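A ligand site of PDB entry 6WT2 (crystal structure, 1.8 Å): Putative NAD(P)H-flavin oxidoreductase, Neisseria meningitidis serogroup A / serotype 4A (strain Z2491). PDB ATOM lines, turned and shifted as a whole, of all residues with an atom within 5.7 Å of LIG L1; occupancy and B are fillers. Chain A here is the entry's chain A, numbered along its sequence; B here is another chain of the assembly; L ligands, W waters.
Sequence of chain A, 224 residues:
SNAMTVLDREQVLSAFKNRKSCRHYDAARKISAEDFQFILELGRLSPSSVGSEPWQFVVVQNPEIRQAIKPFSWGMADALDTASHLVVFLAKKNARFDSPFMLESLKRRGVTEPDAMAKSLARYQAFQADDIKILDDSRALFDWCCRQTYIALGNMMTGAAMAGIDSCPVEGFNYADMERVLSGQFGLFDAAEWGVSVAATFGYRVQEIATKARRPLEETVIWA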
ATOM      1  N   ARG A  19      25.159  -2.902 -19.139  1.00  0.00           N
ATOM      2  CA  ARG A  19      23.734  -3.184 -19.289  1.00  0.00           C
ATOM      3  C   ARG A  19      22.908  -2.186 -18.490  1.00  0.00           C
ATOM      4  O   ARG A  19      23.040  -2.084 -17.266  1.00  0.00           O
ATOM      5  CB  ARG A  19      23.372  -4.603 -18.863  1.00  0.00           C
ATOM      6  CG  ARG A  19      22.047  -5.064 -19.502  1.00  0.00           C
ATOM      7  CD  ARG A  19      21.161  -5.893 -18.548  1.00  0.00           C
ATOM      8  NE  ARG A  19      21.156  -5.317 -17.209  1.00  0.00           N
ATOM      9  CZ  ARG A  19      20.294  -4.395 -16.769  1.00  0.00           C
ATOM     10  NH1 ARG A  19      19.323  -3.931 -17.559  1.00  0.00           N
ATOM     11  NH2 ARG A  19      20.403  -3.924 -15.532  1.00  0.00           N
ATOM     12  N   LYS A  20      22.055  -1.457 -19.202  1.00  0.00           N
ATOM     13  CA  LYS A  20      21.100  -0.539 -18.602  1.00  0.00           C
ATOM     14  C   LYS A  20      19.805  -0.706 -19.380  1.00  0.00           C
ATOM     15  O   LYS A  20      19.833  -0.917 -20.585  1.00  0.00           O
ATOM     16  CB  LYS A  20      21.579   0.911 -18.664  1.00  0.00           C
ATOM     17  CG  LYS A  20      23.001   1.118 -18.167  1.00  0.00           C
ATOM     18  CD  LYS A  20      23.458   2.537 -18.399  1.00  0.00           C
ATOM     19  CE  LYS A  20      24.783   2.822 -17.717  1.00  0.00           C
ATOM     20  NZ  LYS A  20      24.993   4.295 -17.594  1.00  0.00           N
ATOM     21  N   SER A  21      18.672  -0.628 -18.685  1.00  0.00           N
ATOM     22  CA  SER A  21      17.409  -0.756 -19.408  1.00  0.00           C
ATOM     23  C   SER A  21      17.227   0.441 -20.331  1.00  0.00           C
ATOM     24  O   SER A  21      17.341   1.589 -19.919  1.00  0.00           O
ATOM     25  CB  SER A  21      16.250  -0.879 -18.435  1.00  0.00           C
ATOM     26  OG  SER A  21      16.288  -2.155 -17.807  1.00  0.00           O
ATOM     27  N   ARG A  23      14.764   2.346 -23.080  1.00  0.00           N
ATOM     28  CA  ARG A  23      13.392   2.450 -23.562  1.00  0.00           C
ATOM     29  C   ARG A  23      13.284   3.101 -24.941  1.00  0.00           C
ATOM     30  O   ARG A  23      12.216   3.023 -25.548  1.00  0.00           O
ATOM     31  CB  ARG A  23      12.523   3.228 -22.572  1.00  0.00           C
ATOM     32  CG  ARG A  23      12.117   2.396 -21.373  1.00  0.00           C
ATOM     33  CD  ARG A  23      13.177   2.446 -20.280  1.00  0.00           C
ATOM     34  NE  ARG A  23      12.788   1.654 -19.123  1.00  0.00           N
ATOM     35  CZ  ARG A  23      13.429   1.683 -17.953  1.00  0.00           C
ATOM     36  NH1 ARG A  23      14.480   2.475 -17.793  1.00  0.00           N
ATOM     37  NH2 ARG A  23      13.018   0.918 -16.953  1.00  0.00           N
ATOM     38  N   GLY A  75       4.408  -1.051 -21.383  1.00  0.00           N
ATOM     39  CA  GLY A  75       5.776  -1.100 -20.898  1.00  0.00           C
ATOM     40  C   GLY A  75       6.847  -0.962 -21.975  1.00  0.00           C
ATOM     41  O   GLY A  75       8.007  -0.712 -21.643  1.00  0.00           O
ATOM     42  N   MET A  76       6.486  -1.143 -23.251  1.00  0.00           N
ATOM     43  CA  MET A  76       7.445  -1.005 -24.331  1.00  0.00           C
ATOM     44  C   MET A  76       6.856  -0.290 -25.560  1.00  0.00           C
ATOM     45  O   MET A  76       7.297  -0.531 -26.689  1.00  0.00           O
ATOM     46  CB  MET A  76       7.980  -2.383 -24.723  1.00  0.00           C
ATOM     47  CG  MET A  76       6.880  -3.355 -25.156  1.00  0.00           C
ATOM     48  SD  MET A  76       7.629  -4.960 -26.005  1.00  0.00           S
ATOM     49  CE  MET A  76       5.990  -6.033 -26.123  1.00  0.00           C
ATOM     50  N   TYR A 150      13.727 -16.892 -17.197  1.00  0.00           N
ATOM     51  CA  TYR A 150      14.351 -15.658 -16.745  1.00  0.00           C
ATOM     52  C   TYR A 150      15.871 -15.804 -16.638  1.00  0.00           C
ATOM     53  O   TYR A 150      16.584 -14.790 -16.645  1.00  0.00           O
ATOM     54  CB  TYR A 150      13.741 -15.218 -15.412  1.00  0.00           C
ATOM     55  CG  TYR A 150      12.430 -14.450 -15.520  1.00  0.00           C
ATOM     56  CD1 TYR A 150      12.323 -13.133 -15.066  1.00  0.00           C
ATOM     57  CD2 TYR A 150      11.295 -15.037 -16.074  1.00  0.00           C
ATOM     58  CE1 TYR A 150      11.117 -12.427 -15.146  1.00  0.00           C
ATOM     59  CE2 TYR A 150      10.099 -14.341 -16.164  1.00  0.00           C
ATOM     60  CZ  TYR A 150      10.012 -13.048 -15.707  1.00  0.00           C
ATOM     61  OH  TYR A 150       8.817 -12.365 -15.803  1.00  0.00           O
ATOM     62  N   LEU A 153      16.725 -15.069 -20.221  1.00  0.00           N
ATOM     63  CA  LEU A 153      16.569 -13.618 -20.354  1.00  0.00           C
ATOM     64  C   LEU A 153      17.782 -12.880 -19.799  1.00  0.00           C
ATOM     65  O   LEU A 153      18.389 -12.046 -20.492  1.00  0.00           O
ATOM     66  CB  LEU A 153      15.297 -13.178 -19.635  1.00  0.00           C
ATOM     67  CG  LEU A 153      15.125 -11.665 -19.468  1.00  0.00           C
ATOM     68  CD1 LEU A 153      14.674 -11.072 -20.776  1.00  0.00           C
ATOM     69  CD2 LEU A 153      14.146 -11.369 -18.346  1.00  0.00           C
ATOM     70  N   MET A 157      20.577 -10.635 -22.188  1.00  0.00           N
ATOM     71  CA  MET A 157      20.756  -9.188 -21.992  1.00  0.00           C
ATOM     72  C   MET A 157      22.162  -8.806 -21.522  1.00  0.00           C
ATOM     73  O   MET A 157      22.734  -7.812 -21.979  1.00  0.00           O
ATOM     74  CB  MET A 157      19.737  -8.655 -21.001  1.00  0.00           C
ATOM     75  CG  MET A 157      18.323  -8.734 -21.526  1.00  0.00           C
ATOM     76  SD  MET A 157      17.129  -7.865 -20.305  1.00  0.00           S
ATOM     77  CE  MET A 157      17.608  -8.898 -18.699  1.00  0.00           C
ATOM     78  N   CYS A 168      16.225  -4.090 -23.068  1.00  0.00           N
ATOM     79  CA  CYS A 168      15.312  -3.789 -21.943  1.00  0.00           C
ATOM     80  C   CYS A 168      14.484  -5.048 -21.693  1.00  0.00           C
ATOM     81  O   CYS A 168      13.902  -5.583 -22.647  1.00  0.00           O
ATOM     82  CB  CYS A 168      14.386  -2.605 -22.209  1.00  0.00           C
ATOM     83  SG  CYS A 168      13.456  -2.020 -20.735  1.00  0.00           S
ATOM     84  N   PRO A 169      14.415  -5.541 -20.457  1.00  0.00           N
ATOM     85  CA  PRO A 169      13.453  -6.591 -20.139  1.00  0.00           C
ATOM     86  C   PRO A 169      12.060  -5.987 -19.999  1.00  0.00           C
ATOM     87  O   PRO A 169      11.903  -4.815 -19.643  1.00  0.00           O
ATOM     88  CB  PRO A 169      13.954  -7.140 -18.783  1.00  0.00           C
ATOM     89  CG  PRO A 169      15.011  -6.110 -18.273  1.00  0.00           C
ATOM     90  CD  PRO A 169      15.038  -4.966 -19.244  1.00  0.00           C
ATOM     91  N   VAL A 170      11.038  -6.778 -20.321  1.00  0.00           N
ATOM     92  CA  VAL A 170       9.682  -6.222 -20.415  1.00  0.00           C
ATOM     93  C   VAL A 170       8.663  -7.204 -19.842  1.00  0.00           C
ATOM     94  O   VAL A 170       8.482  -8.310 -20.373  1.00  0.00           O
ATOM     95  CB  VAL A 170       9.282  -5.879 -21.864  1.00  0.00           C
ATOM     96  CG1 VAL A 170       7.838  -5.351 -21.891  1.00  0.00           C
ATOM     97  CG2 VAL A 170      10.231  -4.830 -22.454  1.00  0.00           C
ATOM     98  N   GLU A 171       7.965  -6.771 -18.780  1.00  0.00           N
ATOM     99  CA  GLU A 171       6.753  -7.418 -18.291  1.00  0.00           C
ATOM    100  C   GLU A 171       5.520  -6.545 -18.491  1.00  0.00           C
ATOM    101  O   GLU A 171       4.405  -7.004 -18.218  1.00  0.00           O
ATOM    102  CB  GLU A 171       6.872  -7.757 -16.789  1.00  0.00           C
ATOM    103  CG  GLU A 171       7.659  -9.016 -16.479  1.00  0.00           C
ATOM    104  CD  GLU A 171       7.901  -9.161 -14.973  1.00  0.00           C
ATOM    105  OE1 GLU A 171       7.453  -8.273 -14.224  1.00  0.00           O
ATOM    106  OE2 GLU A 171       8.542 -10.136 -14.542  1.00  0.00           O
ATOM    107  N   GLY A 172       5.693  -5.306 -18.942  1.00  0.00           N
ATOM    108  CA  GLY A 172       4.600  -4.357 -18.977  1.00  0.00           C
ATOM    109  C   GLY A 172       3.657  -4.538 -20.152  1.00  0.00           C
ATOM    110  O   GLY A 172       3.606  -3.694 -21.057  1.00  0.00           O
ATOM    111  N   PHE A 173       2.909  -5.620 -20.143  1.00  0.00           N
ATOM    112  CA  PHE A 173       1.903  -5.852 -21.172  1.00  0.00           C
ATOM    113  C   PHE A 173       0.811  -6.729 -20.597  1.00  0.00           C
ATOM    114  O   PHE A 173       1.009  -7.425 -19.600  1.00  0.00           O
ATOM    115  CB  PHE A 173       2.509  -6.482 -22.422  1.00  0.00           C
ATOM    116  CG  PHE A 173       3.315  -7.731 -22.143  1.00  0.00           C
ATOM    117  CD1 PHE A 173       2.694  -8.975 -22.098  1.00  0.00           C
ATOM    118  CD2 PHE A 173       4.690  -7.673 -21.974  1.00  0.00           C
ATOM    119  CE1 PHE A 173       3.419 -10.125 -21.867  1.00  0.00           C
ATOM    120  CE2 PHE A 173       5.424  -8.820 -21.747  1.00  0.00           C
ATOM    121  CZ  PHE A 173       4.793 -10.055 -21.691  1.00  0.00           C
ATOM    122  N   VAL A 198       7.752 -13.609 -20.500  1.00  0.00           N
ATOM    123  CA  VAL A 198       8.427 -12.318 -20.368  1.00  0.00           C
ATOM    124  C   VAL A 198       8.870 -11.910 -21.761  1.00  0.00           C
ATOM    125  O   VAL A 198       8.868 -12.733 -22.688  1.00  0.00           O
ATOM    126  CB  VAL A 198       9.622 -12.423 -19.386  1.00  0.00           C
ATOM    127  CG1 VAL A 198      10.703 -13.314 -19.986  1.00  0.00           C
ATOM    128  CG2 VAL A 198      10.167 -11.028 -18.962  1.00  0.00           C
ATOM    129  N   ILE A 209      22.087   6.856 -21.137  1.00  0.00           N
ATOM    130  CA  ILE A 209      21.217   6.336 -20.083  1.00  0.00           C
ATOM    131  C   ILE A 209      21.988   6.411 -18.768  1.00  0.00           C
ATOM    132  O   ILE A 209      23.110   5.911 -18.665  1.00  0.00           O
ATOM    133  CB  ILE A 209      20.791   4.889 -20.378  1.00  0.00           C
ATOM    134  CG1 ILE A 209      20.088   4.799 -21.728  1.00  0.00           C
ATOM    135  CG2 ILE A 209      19.909   4.352 -19.248  1.00  0.00           C
ATOM    136  CD1 ILE A 209      20.054   3.396 -22.299  1.00  0.00           C
ATOM    137  N   ALA A 210      21.368   7.035 -17.765  1.00  0.00           N
ATOM    138  CA  ALA A 210      21.986   7.105 -16.450  1.00  0.00           C
ATOM    139  C   ALA A 210      21.941   5.750 -15.749  1.00  0.00           C
ATOM    140  O   ALA A 210      20.960   5.022 -15.853  1.00  0.00           O
ATOM    141  CB  ALA A 210      21.278   8.154 -15.592  1.00  0.00           C
ATOM    142  N   LYS A 212      21.249   3.222 -12.953  1.00  0.00           N
ATOM    143  CA  LYS A 212      20.179   3.207 -11.955  1.00  0.00           C
ATOM    144  C   LYS A 212      20.666   2.620 -10.637  1.00  0.00           C
ATOM    145  O   LYS A 212      21.604   1.820 -10.604  1.00  0.00           O
ATOM    146  CB  LYS A 212      18.974   2.421 -12.494  1.00  0.00           C
ATOM    147  CG  LYS A 212      18.417   2.980 -13.816  1.00  0.00           C
ATOM    148  CD  LYS A 212      18.231   4.496 -13.745  1.00  0.00           C
ATOM    149  CE  LYS A 212      17.463   5.043 -14.929  1.00  0.00           C
ATOM    150  NZ  LYS A 212      18.142   4.781 -16.236  1.00  0.00           N
ATOM    151  N   ALA A 213      20.037   3.043  -9.546  1.00  0.00           N
ATOM    152  CA  ALA A 213      20.495   2.706  -8.202  1.00  0.00           C
ATOM    153  C   ALA A 213      20.199   1.244  -7.866  1.00  0.00           C
ATOM    154  O   ALA A 213      19.335   0.605  -8.475  1.00  0.00           O
ATOM    155  CB  ALA A 213      19.823   3.595  -7.163  1.00  0.00           C
ATOM    156  N   ARG A 214      20.934   0.727  -6.894  1.00  0.00           N
ATOM    157  CA  ARG A 214      20.659  -0.565  -6.286  1.00  0.00           C
ATOM    158  C   ARG A 214      20.777  -0.426  -4.774  1.00  0.00           C
ATOM    159  O   ARG A 214      21.517   0.424  -4.277  1.00  0.00           O
ATOM    160  CB  ARG A 214      21.631  -1.668  -6.777  1.00  0.00           C
ATOM    161  CG  ARG A 214      21.485  -2.019  -8.257  1.00  0.00           C
ATOM    162  CD  ARG A 214      20.127  -2.645  -8.550  1.00  0.00           C
ATOM    163  NE  ARG A 214      20.089  -3.208  -9.904  1.00  0.00           N
ATOM    164  CZ  ARG A 214      19.869  -2.479 -10.995  1.00  0.00           C
ATOM    165  NH1 ARG A 214      19.643  -1.169 -10.892  1.00  0.00           N
ATOM    166  NH2 ARG A 214      19.850  -3.060 -12.194  1.00  0.00           N
ATOM    167  N   LEU B  45      23.617  -5.989  -8.878  1.00  0.00           N
ATOM    168  CA  LEU B  45      23.432  -5.120 -10.031  1.00  0.00           C
ATOM    169  C   LEU B  45      22.431  -5.669 -11.053  1.00  0.00           C
ATOM    170  O   LEU B  45      22.174  -4.995 -12.048  1.00  0.00           O
ATOM    171  CB  LEU B  45      24.781  -4.890 -10.710  1.00  0.00           C
ATOM    172  CG  LEU B  45      25.795  -4.060  -9.939  1.00  0.00           C
ATOM    173  CD1 LEU B  45      27.095  -3.942 -10.718  1.00  0.00           C
ATOM    174  CD2 LEU B  45      25.227  -2.672  -9.629  1.00  0.00           C
ATOM    175  N   PRO B  47      19.043  -6.574 -13.138  1.00  0.00           N
ATOM    176  CA  PRO B  47      17.746  -5.882 -13.265  1.00  0.00           C
ATOM    177  C   PRO B  47      16.632  -6.663 -12.587  1.00  0.00           C
ATOM    178  O   PRO B  47      16.754  -7.864 -12.295  1.00  0.00           O
ATOM    179  CB  PRO B  47      17.533  -5.817 -14.782  1.00  0.00           C
ATOM    180  CG  PRO B  47      18.241  -7.073 -15.300  1.00  0.00           C
ATOM    181  CD  PRO B  47      19.472  -7.219 -14.400  1.00  0.00           C
ATOM    182  N   SER B  48      15.527  -5.979 -12.356  1.00  0.00           N
ATOM    183  CA  SER B  48      14.355  -6.585 -11.727  1.00  0.00           C
ATOM    184  C   SER B  48      13.140  -5.758 -12.124  1.00  0.00           C
ATOM    185  O   SER B  48      13.241  -4.551 -12.346  1.00  0.00           O
ATOM    186  CB  SER B  48      14.490  -6.665 -10.194  1.00  0.00           C
ATOM    187  OG  SER B  48      14.685  -5.368  -9.627  1.00  0.00           O
ATOM    188  N   SER B  49      11.999  -6.439 -12.235  1.00  0.00           N
ATOM    189  CA  SER B  49      10.748  -5.741 -12.531  1.00  0.00           C
ATOM    190  C   SER B  49      10.536  -4.582 -11.562  1.00  0.00           C
ATOM    191  O   SER B  49      10.682  -4.732 -10.346  1.00  0.00           O
ATOM    192  CB  SER B  49       9.571  -6.721 -12.466  1.00  0.00           C
ATOM    193  OG  SER B  49       8.346  -6.101 -12.839  1.00  0.00           O
ATOM    194  N   VAL B  50      10.173  -3.409 -12.107  1.00  0.00           N
ATOM    195  CA  VAL B  50      10.025  -2.109 -11.449  1.00  0.00           C
ATOM    196  C   VAL B  50      11.165  -1.758 -10.501  1.00  0.00           C
ATOM    197  O   VAL B  50      10.996  -0.923  -9.610  1.00  0.00           O
ATOM    198  CB  VAL B  50       8.668  -1.990 -10.732  1.00  0.00           C
ATOM    199  CG1 VAL B  50       7.515  -2.352 -11.662  1.00  0.00           C
ATOM    200  CG2 VAL B  50       8.605  -2.819  -9.440  1.00  0.00           C
ATOM    201  N   GLY B  51      12.355  -2.308 -10.728  1.00  0.00           N
ATOM    202  CA  GLY B  51      13.444  -2.038  -9.801  1.00  0.00           C
ATOM    203  C   GLY B  51      13.172  -2.532  -8.401  1.00  0.00           C
ATOM    204  O   GLY B  51      13.674  -1.955  -7.419  1.00  0.00           O
ATOM    205  N   ARG B 109      14.120   4.478  -7.185  1.00  0.00           N
ATOM    206  CA  ARG B 109      14.066   4.821  -8.596  1.00  0.00           C
ATOM    207  C   ARG B 109      14.092   6.329  -8.821  1.00  0.00           C
ATOM    208  O   ARG B 109      14.098   6.764  -9.974  1.00  0.00           O
ATOM    209  CB  ARG B 109      12.800   4.258  -9.245  1.00  0.00           C
ATOM    210  CG  ARG B 109      12.694   2.736  -9.246  1.00  0.00           C
ATOM    211  CD  ARG B 109      11.550   2.258 -10.125  1.00  0.00           C
ATOM    212  NE  ARG B 109      11.907   2.318 -11.541  1.00  0.00           N
ATOM    213  CZ  ARG B 109      11.118   1.894 -12.524  1.00  0.00           C
ATOM    214  NH1 ARG B 109       9.916   1.406 -12.239  1.00  0.00           N
ATOM    215  NH2 ARG B 109      11.517   1.965 -13.791  1.00  0.00           N
ATOM    216  N   GLN B 148      12.365 -12.917 -10.669  1.00  0.00           N
ATOM    217  CA  GLN B 148      13.439 -11.929 -10.676  1.00  0.00           C
ATOM    218  C   GLN B 148      14.738 -12.512 -10.106  1.00  0.00           C
ATOM    219  O   GLN B 148      15.824 -12.230 -10.624  1.00  0.00           O
ATOM    220  CB  GLN B 148      13.035 -10.686  -9.862  1.00  0.00           C
ATOM    221  CG  GLN B 148      11.589 -10.186 -10.032  1.00  0.00           C
ATOM    222  CD  GLN B 148      11.214  -9.934 -11.487  1.00  0.00           C
ATOM    223  OE1 GLN B 148      11.965  -9.291 -12.236  1.00  0.00           O
ATOM    224  NE2 GLN B 148      10.045 -10.425 -11.881  1.00  0.00           N
ATOM    225  N   ILE B 151      17.064 -14.181 -12.490  1.00  0.00           N
ATOM    226  CA  ILE B 151      17.927 -13.289 -13.252  1.00  0.00           C
ATOM    227  C   ILE B 151      19.255 -13.098 -12.514  1.00  0.00           C
ATOM    228  O   ILE B 151      20.327 -13.185 -13.112  1.00  0.00           O
ATOM    229  CB  ILE B 151      17.245 -11.927 -13.496  1.00  0.00           C
ATOM    230  CG1 ILE B 151      15.937 -12.074 -14.265  1.00  0.00           C
ATOM    231  CG2 ILE B 151      18.180 -10.995 -14.214  1.00  0.00           C
ATOM    232  CD1 ILE B 151      15.194 -10.726 -14.389  1.00  0.00           C
HETATM  233  N1  LIG L   1      11.211  -1.499 -18.012  1.00  0.00           N
HETATM  234  C1  LIG L   1      10.213  -0.914 -18.720  1.00  0.00           C
HETATM  235  O1  LIG L   1      10.370   0.279 -19.072  1.00  0.00           O
HETATM  236  N2  LIG L   1       9.092  -1.552 -19.072  1.00  0.00           N
HETATM  237  C2  LIG L   1       8.832  -2.810 -18.690  1.00  0.00           C
HETATM  238  O2  LIG L   1       7.815  -3.441 -19.083  1.00  0.00           O
HETATM  239  C3  LIG L   1       9.862  -3.516 -17.902  1.00  0.00           C
HETATM  240  N3  LIG L   1       9.614  -4.739 -17.404  1.00  0.00           N
HETATM  241  C4  LIG L   1      10.603  -5.424 -16.767  1.00  0.00           C
HETATM  242  C5  LIG L   1      10.466  -6.790 -16.554  1.00  0.00           C
HETATM  243  C6  LIG L   1      11.466  -7.487 -15.894  1.00  0.00           C
HETATM  244  C7  LIG L   1      11.335  -8.972 -15.639  1.00  0.00           C
HETATM  245  C8  LIG L   1      12.706  -6.786 -15.476  1.00  0.00           C
HETATM  246  C9  LIG L   1      13.838  -7.576 -14.861  1.00  0.00           C
HETATM  247  C10 LIG L   1      12.879  -5.433 -15.750  1.00  0.00           C
HETATM  248  C11 LIG L   1      11.889  -4.741 -16.443  1.00  0.00           C
HETATM  249  N4  LIG L   1      12.061  -3.382 -16.774  1.00  0.00           N
HETATM  250  C12 LIG L   1      11.037  -2.725 -17.467  1.00  0.00           C
HETATM  251  C13 LIG L   1      13.310  -2.679 -16.447  1.00  0.00           C
HETATM  252  C14 LIG L   1      13.379  -2.259 -14.971  1.00  0.00           C
HETATM  253  O3  LIG L   1      12.542  -1.107 -14.700  1.00  0.00           O
HETATM  254  C15 LIG L   1      14.853  -2.001 -14.650  1.00  0.00           C
HETATM  255  O4  LIG L   1      15.572  -3.244 -14.801  1.00  0.00           O
HETATM  256  C16 LIG L   1      15.150  -1.467 -13.245  1.00  0.00           C
HETATM  257  O5  LIG L   1      14.445  -0.250 -13.044  1.00  0.00           O
HETATM  258  C17 LIG L   1      16.637  -1.241 -13.059  1.00  0.00           C
HETATM  259  O6  LIG L   1      17.154  -0.338 -14.027  1.00  0.00           O
HETATM  260  P1  LIG L   1      18.393  -0.810 -14.945  1.00  0.00           P
HETATM  261  O7  LIG L   1      17.887  -2.130 -15.475  1.00  0.00           O
HETATM  262  O8  LIG L   1      18.627   0.223 -16.008  1.00  0.00           O
HETATM  263  O9  LIG L   1      19.578  -1.031 -14.050  1.00  0.00           O
HETATM  264  N1  LG2 L   2       5.886  -1.795 -16.369  1.00  0.00           N
HETATM  265  C1  LG2 L   2       7.043  -1.220 -16.058  1.00  0.00           C
HETATM  266  C2  LG2 L   2       7.987  -1.930 -15.323  1.00  0.00           C
HETATM  267  C3  LG2 L   2       7.731  -3.219 -14.897  1.00  0.00           C
HETATM  268  C4  LG2 L   2       6.511  -3.790 -15.226  1.00  0.00           C
HETATM  269  C5  LG2 L   2       5.598  -3.048 -15.970  1.00  0.00           C
HETATM  270  C6  LG2 L   2       9.287  -1.288 -14.965  1.00  0.00           C
HETATM  271  O1  LG2 L   2      10.175  -2.002 -14.500  1.00  0.00           O
HETATM  272  O2  LG2 L   2       9.447  -0.064 -15.165  1.00  0.00           O
HETATM  273  O   HOH W   1      15.412   1.612 -15.293  1.00  0.00           O
HETATM  274  O   HOH W   2       8.497   1.971 -19.998  1.00  0.00           O
HETATM  275  O   HOH W   3      22.564  -0.581 -14.208  1.00  0.00           O
HETATM  276  O   HOH W   4      21.183   1.346 -15.089  1.00  0.00           O
HETATM  277  O   HOH W   5      17.696   2.281 -17.092  1.00  0.00           O
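Water W5 lies within hydrogen-bond range of an oxygen (O8) of LIG L1 (2.5 Å), the side-chain amino group of Lys 212 (2.7 Å), the backbone carbonyl oxygen of Ser 21 (2.9 Å) and the guanidinium group of Arg 23 (3.3 Å). Water W2 bridges O1 of LIG L1 (2.7 Å) and O of Gly 75 (3.2 Å). Water W1 lies within hydrogen-bond range of the guanidinium group (NH1) of Arg 23 (2.8 Å) and an oxygen (O6) of LIG L1 (2.9 Å). Water W4 bridges the backbone NH of Lys 212 (2.8 Å) and an oxygen (O8) of LIG L1 (2.9 Å). Water W3 lies within hydrogen-bond range of an oxygen (O9) of LIG L1 (3.0 Å) and the backbone carbonyl oxygen (O) of Arg 19 (3.4 Å).
The backbone carbonyl oxygen of Pro 169 lies close to a nitrogen (N3) of LIG L1, at 3.2 Å. CA of Lys 20 touches O8 of LIG L1 (3.7 Å). Tyr 150 touches LIG L1. Val 170 touches LIG L1. Lys 212 touches LIG L1. Pro 47 of chain B touches LIG L1. Ser 48 of chain B touches LIG L1 (CA to C9, 3.3 Å). Ser 49 of chain B touches LIG L1 (N to C8, 3.3 Å). Gly 51 of chain B touches LIG L1. Gln 148 of chain B touches LIG L1. Ile 151 of chain B touches LIG L1 (CD1 to C9, 3.5 Å). Hydrophobic or aromatic side chains within 4 Å of LIG L1: Tyr 150, Pro 169, Val 170, Pro 47 of chain B and Ile 151 of chain B. Of the 30 residues printed, 20 come within 4 Å of LIG L1. The nearest printed residue that does not touch LIG L1 is Val 198 (4.1 Å).
An oxygen (O1) of LG2 L2 sits at hydrogen-bond distance from the backbone NH (N) of Val 50 of chain B, at 2.8 Å. O7 of LIG L1 lies within hydrogen-bond range of OG of Ser 21, at 2.8 Å. The backbone NH of Ser 21 sits at hydrogen-bond distance from an oxygen (O8) of LIG L1. An oxygen (O2) of LIG L1 sits at hydrogen-bond distance from the backbone NH (N) of Gly 172, at 2.8 Å. The guanidinium group of Arg 23 sits at hydrogen-bond distance from an oxygen (O1) of LIG L1 (2.8 Å). The guanidinium group of Arg 214 lies within salt-bridge range of an oxygen (O9) of LIG L1 (2.8 Å). The guanidinium group (NH2) of Arg 109 of chain B lies within hydrogen-bond range of an oxygen (O3) of LIG L1 (3.4 Å). An oxygen (O7) of LIG L1 is in salt-bridge range of the guanidinium group (NH2) of Arg 19 (3.1 Å). O2 of LG2 L2 is in salt-bridge range of NH2 of Arg 109 of chain B, 3.2 Å away. The side-chain sulfur (SG) of Cys 168 is in hydrogen-bond range of a nitrogen (N1) of LIG L1. N of Glu 171 sits at hydrogen-bond distance from N3 of LIG L1 (3.0 Å). O of Gly 75 is in hydrogen-bond range of N2 of LIG L1 (2.9 Å).
O of Leu 45 of chain B sits at hydrogen-bond distance from NH2 of Arg 214, at 3.0 Å. The side-chain carboxylate of Glu 171 lies within hydrogen-bond range of the side-chain amide nitrogen of Gln 148 of chain B, 3.1 Å away. O of Gly 172 lies within hydrogen-bond range of N of Gly 75. O of Ala 210 sits at hydrogen-bond distance from NZ of Lys 212 (2.9 Å). The side-chain amino group of Lys 20 is in hydrogen-bond range of the backbone carbonyl oxygen of Ile 209 (2.7 Å). OE1 of Glu 171 lies within hydrogen-bond range of OG of Ser 49 of chain B (2.7 Å). The side-chain amide oxygen of Gln 148 of chain B lies within hydrogen-bond range of the backbone NH of Ser 49 of chain B (2.9 Å). OH of Tyr 150 lies within hydrogen-bond range of OE2 of Glu 171 (2.6 Å).
O1 of LG2 L2 lies within hydrogen-bond range of O3 of LIG L1, 2.5 Å away.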
